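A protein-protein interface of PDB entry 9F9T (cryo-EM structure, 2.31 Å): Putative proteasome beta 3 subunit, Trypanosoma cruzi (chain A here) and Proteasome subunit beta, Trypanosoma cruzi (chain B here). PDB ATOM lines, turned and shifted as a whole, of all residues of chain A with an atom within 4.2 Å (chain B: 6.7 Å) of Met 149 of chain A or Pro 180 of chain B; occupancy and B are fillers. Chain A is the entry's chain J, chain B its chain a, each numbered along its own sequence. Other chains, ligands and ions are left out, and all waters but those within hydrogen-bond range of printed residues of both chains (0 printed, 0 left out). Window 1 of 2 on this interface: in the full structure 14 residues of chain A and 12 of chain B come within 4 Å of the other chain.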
ATOM      1  N   SER A 145     -23.488   4.054  27.967  1.00  0.00           N
ATOM      2  CA  SER A 145     -23.547   4.620  26.641  1.00  0.00           C
ATOM      3  C   SER A 145     -23.193   3.599  25.575  1.00  0.00           C
ATOM      4  O   SER A 145     -23.108   3.945  24.407  1.00  0.00           O
ATOM      5  CB  SER A 145     -22.639   5.818  26.536  1.00  0.00           C
ATOM      6  OG  SER A 145     -23.152   6.947  27.232  1.00  0.00           O
ATOM      7  N   LEU A 146     -22.955   2.360  25.975  1.00  0.00           N
ATOM      8  CA  LEU A 146     -22.449   1.320  25.088  1.00  0.00           C
ATOM      9  C   LEU A 146     -23.563   0.338  24.725  1.00  0.00           C
ATOM     10  O   LEU A 146     -23.694   0.000  23.558  1.00  0.00           O
ATOM     11  CB  LEU A 146     -21.312   0.584  25.789  1.00  0.00           C
ATOM     12  CG  LEU A 146     -19.947   1.126  25.445  1.00  0.00           C
ATOM     13  CD1 LEU A 146     -18.875   0.213  25.995  1.00  0.00           C
ATOM     14  CD2 LEU A 146     -19.819   1.273  23.943  1.00  0.00           C
ATOM     15  N   HIS A 147     -24.232  -0.182  25.750  1.00  0.00           N
ATOM     16  CA  HIS A 147     -25.608  -0.659  25.692  1.00  0.00           C
ATOM     17  C   HIS A 147     -26.370  -0.082  24.490  1.00  0.00           C
ATOM     18  O   HIS A 147     -26.552  -0.785  23.497  1.00  0.00           O
ATOM     19  CB  HIS A 147     -26.245  -0.604  27.099  1.00  0.00           C
ATOM     20  CG  HIS A 147     -25.636  -1.640  27.978  1.00  0.00           C
ATOM     21  ND1 HIS A 147     -25.060  -1.454  29.209  1.00  0.00           N
ATOM     22  CD2 HIS A 147     -25.484  -2.969  27.706  1.00  0.00           C
ATOM     23  CE1 HIS A 147     -24.556  -2.624  29.655  1.00  0.00           C
ATOM     24  NE2 HIS A 147     -24.815  -3.564  28.761  1.00  0.00           N
ATOM     25  N   GLY A 148     -26.823   1.163  24.522  1.00  0.00           N
ATOM     26  CA  GLY A 148     -27.639   1.676  23.423  1.00  0.00           C
ATOM     27  C   GLY A 148     -26.932   1.778  22.059  1.00  0.00           C
ATOM     28  O   GLY A 148     -27.584   1.786  21.011  1.00  0.00           O
ATOM     29  N   MET A 149     -25.611   1.884  22.017  1.00  0.00           N
ATOM     30  CA  MET A 149     -24.977   1.903  20.711  1.00  0.00           C
ATOM     31  C   MET A 149     -25.101   0.528  20.040  1.00  0.00           C
ATOM     32  O   MET A 149     -25.448   0.373  18.878  1.00  0.00           O
ATOM     33  CB  MET A 149     -23.492   2.249  20.895  1.00  0.00           C
ATOM     34  CG  MET A 149     -23.252   3.711  21.267  1.00  0.00           C
ATOM     35  SD  MET A 149     -23.676   4.891  19.957  1.00  0.00           S
ATOM     36  CE  MET A 149     -23.124   4.074  18.446  1.00  0.00           C
ATOM     37  N   CYS A 150     -24.787  -0.488  20.823  1.00  0.00           N
ATOM     38  CA  CYS A 150     -24.869  -1.868  20.407  1.00  0.00           C
ATOM     39  C   CYS A 150     -26.291  -2.355  20.143  1.00  0.00           C
ATOM     40  O   CYS A 150     -26.454  -3.137  19.219  1.00  0.00           O
ATOM     41  CB  CYS A 150     -24.278  -2.709  21.511  1.00  0.00           C
ATOM     42  SG  CYS A 150     -22.587  -2.215  21.871  1.00  0.00           S
ATOM     43  N   GLU A 151     -27.291  -1.950  20.944  1.00  0.00           N
ATOM     44  CA  GLU A 151     -28.681  -2.348  20.683  1.00  0.00           C
ATOM     45  C   GLU A 151     -29.097  -1.848  19.309  1.00  0.00           C
ATOM     46  O   GLU A 151     -29.688  -2.591  18.555  1.00  0.00           O
ATOM     47  CB  GLU A 151     -29.663  -1.851  21.748  1.00  0.00           C
ATOM     48  CG  GLU A 151     -31.123  -2.336  21.624  1.00  0.00           C
ATOM     49  CD  GLU A 151     -31.438  -3.796  21.950  1.00  0.00           C
ATOM     50  OE1 GLU A 151     -32.608  -4.223  21.702  1.00  0.00           O
ATOM     51  OE2 GLU A 151     -30.520  -4.520  22.441  1.00  0.00           O
ATOM     52  N   ALA A 152     -28.613  -0.663  18.912  1.00  0.00           N
ATOM     53  CA  ALA A 152     -28.990  -0.094  17.623  1.00  0.00           C
ATOM     54  C   ALA A 152     -28.091  -0.451  16.453  1.00  0.00           C
ATOM     55  O   ALA A 152     -28.455  -0.181  15.325  1.00  0.00           O
ATOM     56  CB  ALA A 152     -29.053   1.396  17.725  1.00  0.00           C
ATOM     57  N   LEU A 153     -26.887  -0.955  16.674  1.00  0.00           N
ATOM     58  CA  LEU A 153     -26.025  -1.274  15.539  1.00  0.00           C
ATOM     59  C   LEU A 153     -25.872  -2.779  15.356  1.00  0.00           C
ATOM     60  O   LEU A 153     -25.646  -3.237  14.232  1.00  0.00           O
ATOM     61  CB  LEU A 153     -24.690  -0.603  15.785  1.00  0.00           C
ATOM     62  CG  LEU A 153     -24.726   0.920  15.744  1.00  0.00           C
ATOM     63  CD1 LEU A 153     -23.392   1.486  16.212  1.00  0.00           C
ATOM     64  CD2 LEU A 153     -25.035   1.385  14.341  1.00  0.00           C
ATOM     65  N   ALA A 170     -19.088   1.879  17.967  1.00  0.00           N
ATOM     66  CA  ALA A 170     -19.654   1.880  19.307  1.00  0.00           C
ATOM     67  C   ALA A 170     -18.678   2.484  20.306  1.00  0.00           C
ATOM     68  O   ALA A 170     -18.989   3.449  20.982  1.00  0.00           O
ATOM     69  CB  ALA A 170     -20.013   0.472  19.762  1.00  0.00           C
ATOM     70  N   SER A 173     -17.973   6.465  19.661  1.00  0.00           N
ATOM     71  CA  SER A 173     -19.076   7.307  20.057  1.00  0.00           C
ATOM     72  C   SER A 173     -19.292   7.206  21.566  1.00  0.00           C
ATOM     73  O   SER A 173     -19.670   8.182  22.194  1.00  0.00           O
ATOM     74  CB  SER A 173     -20.335   6.962  19.262  1.00  0.00           C
ATOM     75  OG  SER A 173     -20.011   6.565  17.917  1.00  0.00           O
ATOM     76  N   THR B 170     -31.385  15.348  24.032  1.00  0.00           N
ATOM     77  CA  THR B 170     -32.168  14.324  24.716  1.00  0.00           C
ATOM     78  C   THR B 170     -32.001  14.409  26.215  1.00  0.00           C
ATOM     79  O   THR B 170     -31.049  14.926  26.701  1.00  0.00           O
ATOM     80  CB  THR B 170     -31.796  12.928  24.203  1.00  0.00           C
ATOM     81  OG1 THR B 170     -32.451  11.818  24.812  1.00  0.00           O
ATOM     82  CG2 THR B 170     -30.347  12.753  24.464  1.00  0.00           C
ATOM     83  N   SER B 175     -30.978   8.687  28.332  1.00  0.00           N
ATOM     84  CA  SER B 175     -30.425   9.716  27.478  1.00  0.00           C
ATOM     85  C   SER B 175     -28.946   9.497  27.253  1.00  0.00           C
ATOM     86  O   SER B 175     -28.391  10.047  26.333  1.00  0.00           O
ATOM     87  CB  SER B 175     -30.585  11.082  28.110  1.00  0.00           C
ATOM     88  OG  SER B 175     -29.466  11.377  28.918  1.00  0.00           O
ATOM     89  N   SER B 176     -28.318   8.792  28.202  1.00  0.00           N
ATOM     90  CA  SER B 176     -26.905   8.478  28.130  1.00  0.00           C
ATOM     91  C   SER B 176     -26.657   7.336  27.165  1.00  0.00           C
ATOM     92  O   SER B 176     -25.500   7.148  26.827  1.00  0.00           O
ATOM     93  CB  SER B 176     -26.353   8.124  29.465  1.00  0.00           C
ATOM     94  OG  SER B 176     -27.006   6.946  29.848  1.00  0.00           O
ATOM     95  N   PHE B 177     -27.674   6.670  26.628  1.00  0.00           N
ATOM     96  CA  PHE B 177     -27.399   5.902  25.443  1.00  0.00           C
ATOM     97  C   PHE B 177     -28.023   6.440  24.170  1.00  0.00           C
ATOM     98  O   PHE B 177     -27.568   6.058  23.088  1.00  0.00           O
ATOM     99  CB  PHE B 177     -28.149   4.609  25.139  1.00  0.00           C
ATOM    100  CG  PHE B 177     -29.070   3.992  26.129  1.00  0.00           C
ATOM    101  CD1 PHE B 177     -28.629   3.711  27.383  1.00  0.00           C
ATOM    102  CD2 PHE B 177     -30.249   3.461  25.692  1.00  0.00           C
ATOM    103  CE1 PHE B 177     -29.439   3.075  28.288  1.00  0.00           C
ATOM    104  CE2 PHE B 177     -31.079   2.843  26.601  1.00  0.00           C
ATOM    105  CZ  PHE B 177     -30.675   2.678  27.902  1.00  0.00           C
ATOM    106  N   VAL B 178     -29.125   7.165  24.234  1.00  0.00           N
ATOM    107  CA  VAL B 178     -29.668   7.727  23.009  1.00  0.00           C
ATOM    108  C   VAL B 178     -28.701   8.763  22.442  1.00  0.00           C
ATOM    109  O   VAL B 178     -28.654   8.921  21.232  1.00  0.00           O
ATOM    110  CB  VAL B 178     -31.057   8.339  23.252  1.00  0.00           C
ATOM    111  CG1 VAL B 178     -31.626   9.029  22.040  1.00  0.00           C
ATOM    112  CG2 VAL B 178     -32.048   7.311  23.710  1.00  0.00           C
ATOM    113  N   GLU B 179     -27.917   9.450  23.271  1.00  0.00           N
ATOM    114  CA  GLU B 179     -27.188  10.634  22.810  1.00  0.00           C
ATOM    115  C   GLU B 179     -25.948  10.298  22.005  1.00  0.00           C
ATOM    116  O   GLU B 179     -25.768  10.808  20.923  1.00  0.00           O
ATOM    117  CB  GLU B 179     -26.845  11.564  23.958  1.00  0.00           C
ATOM    118  CG  GLU B 179     -26.935  13.013  23.570  1.00  0.00           C
ATOM    119  CD  GLU B 179     -26.680  14.051  24.665  1.00  0.00           C
ATOM    120  OE1 GLU B 179     -26.188  13.680  25.754  1.00  0.00           O
ATOM    121  OE2 GLU B 179     -27.003  15.260  24.413  1.00  0.00           O
ATOM    122  N   PRO B 180     -25.078   9.337  22.392  1.00  0.00           N
ATOM    123  CA  PRO B 180     -24.001   8.907  21.501  1.00  0.00           C
ATOM    124  C   PRO B 180     -24.501   8.337  20.189  1.00  0.00           C
ATOM    125  O   PRO B 180     -23.740   8.292  19.233  1.00  0.00           O
ATOM    126  CB  PRO B 180     -23.223   7.802  22.210  1.00  0.00           C
ATOM    127  CG  PRO B 180     -23.817   7.739  23.582  1.00  0.00           C
ATOM    128  CD  PRO B 180     -24.997   8.681  23.702  1.00  0.00           C
ATOM    129  N   LEU B 181     -25.740   7.843  20.157  1.00  0.00           N
ATOM    130  CA  LEU B 181     -26.204   7.222  18.938  1.00  0.00           C
ATOM    131  C   LEU B 181     -26.533   8.343  17.983  1.00  0.00           C
ATOM    132  O   LEU B 181     -26.156   8.287  16.819  1.00  0.00           O
ATOM    133  CB  LEU B 181     -27.359   6.267  19.222  1.00  0.00           C
ATOM    134  CG  LEU B 181     -28.143   5.741  18.012  1.00  0.00           C
ATOM    135  CD1 LEU B 181     -27.270   4.743  17.250  1.00  0.00           C
ATOM    136  CD2 LEU B 181     -29.489   5.071  18.450  1.00  0.00           C
ATOM    137  N   MET B 182     -27.069   9.431  18.502  1.00  0.00           N
ATOM    138  CA  MET B 182     -27.415  10.525  17.623  1.00  0.00           C
ATOM    139  C   MET B 182     -26.132  11.254  17.232  1.00  0.00           C
ATOM    140  O   MET B 182     -26.015  11.755  16.136  1.00  0.00           O
ATOM    141  CB  MET B 182     -28.298  11.522  18.378  1.00  0.00           C
ATOM    142  CG  MET B 182     -29.764  11.120  18.540  1.00  0.00           C
ATOM    143  SD  MET B 182     -30.442  12.357  19.738  1.00  0.00           S
ATOM    144  CE  MET B 182     -32.165  12.363  19.275  1.00  0.00           C
ATOM    145  N   ASP B 183     -25.174  11.350  18.155  1.00  0.00           N
ATOM    146  CA  ASP B 183     -23.894  11.921  17.809  1.00  0.00           C
ATOM    147  C   ASP B 183     -23.374  11.155  16.600  1.00  0.00           C
ATOM    148  O   ASP B 183     -23.183  11.739  15.549  1.00  0.00           O
ATOM    149  CB  ASP B 183     -22.877  11.919  18.959  1.00  0.00           C
ATOM    150  CG  ASP B 183     -23.049  12.849  20.176  1.00  0.00           C
ATOM    151  OD1 ASP B 183     -23.524  13.990  20.029  1.00  0.00           O
ATOM    152  OD2 ASP B 183     -22.552  12.434  21.278  1.00  0.00           O
ATOM    153  N   CYS B 184     -23.240   9.842  16.724  1.00  0.00           N
ATOM    154  CA  CYS B 184     -22.840   8.955  15.631  1.00  0.00           C
ATOM    155  C   CYS B 184     -23.617   9.217  14.327  1.00  0.00           C
ATOM    156  O   CYS B 184     -23.004   9.472  13.295  1.00  0.00           O
ATOM    157  CB  CYS B 184     -22.926   7.481  16.063  1.00  0.00           C
ATOM    158  SG  CYS B 184     -22.165   6.276  14.928  1.00  0.00           S
ATOM    159  N   LEU B 185     -24.916   9.082  14.293  1.00  0.00           N
ATOM    160  CA  LEU B 185     -25.598   8.991  12.993  1.00  0.00           C
ATOM    161  C   LEU B 185     -25.698  10.364  12.321  1.00  0.00           C
ATOM    162  O   LEU B 185     -25.665  10.434  11.103  1.00  0.00           O
ATOM    163  CB  LEU B 185     -27.001   8.391  13.171  1.00  0.00           C
ATOM    164  CG  LEU B 185     -27.050   7.020  13.866  1.00  0.00           C
ATOM    165  CD1 LEU B 185     -28.492   6.515  14.054  1.00  0.00           C
ATOM    166  CD2 LEU B 185     -26.205   5.987  13.097  1.00  0.00           C
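The side-chain sulfur of Met 149 of chain A lies close to the backbone carbonyl oxygen of Pro 180 of chain B (3.5 Å).
The backbone NH of Leu 181 of chain B sits close to the side-chain sulfur of Met 149 of chain A (3.6 Å).
The side-chain hydroxyl (OG) of Ser 145 of chain A lies close to the backbone carbonyl oxygen (O) of Ser 176 of chain B (2.4 Å).
OG of Ser 173 of chain A lies close to SG of Cys 184 of chain B.
Among the printed residues, merely in contact across the chains: Ser 145 of chain A with Pro 180 of chain B, Gly 148 of chain A with Phe 177 of chain B, Ala 152 of chain A with Leu 181 of chain B and Ser 173 of chain A with Pro 180 of chain B.
Met 149 of chain A touches just these residues of chain B: Pro 180 (3.5 Å) and Leu 181 (3.6 Å).
Of the printed residues of chain B, Ala 152 of chain A touches Leu 181 (3.8 Å).
Printed residues of chain A within 4 Å of Ser 176 of chain B: Ser 145 (2.4 Å).
Of the printed residues of chain A, Phe 177 of chain B touches Gly 148 (3.4 Å).
Pro 180 of chain B touches three residues of chain A.
Of the printed residues of chain A, Cys 184 of chain B touches Ser 173.
The nearest printed residue of chain A that does not touch Pro 180 of chain B is Leu 146 of chain A (6.0 Å).
The nearest printed residue of chain B that does not touch Ser 173 of chain A is Asp 183 of chain B (5.2 Å).
Of the 11 printed residues of chain A, 5 touch a printed residue of chain B.
Printed residues of chain A that touch a printed residue of chain B: Ser 145, Gly 148, Met 149, Ala 152 and Ser 173.
Hydrophobic or aromatic side chains of chain A that line the printed part of chain B: Met 149 and Ala 152.
Of the 12 printed residues of chain B, 5 touch a printed residue of chain A.
Printed residues of chain B that touch a printed residue of chain A: Ser 176, Phe 177, Pro 180, Leu 181 and Cys 184.
Among the printed residues, 8 pairs touch across the chains.
Among the printed residues, no Asp or Glu carboxylate lies within 4 Å of a Lys or Arg side-chain nitrogen of the other chain.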
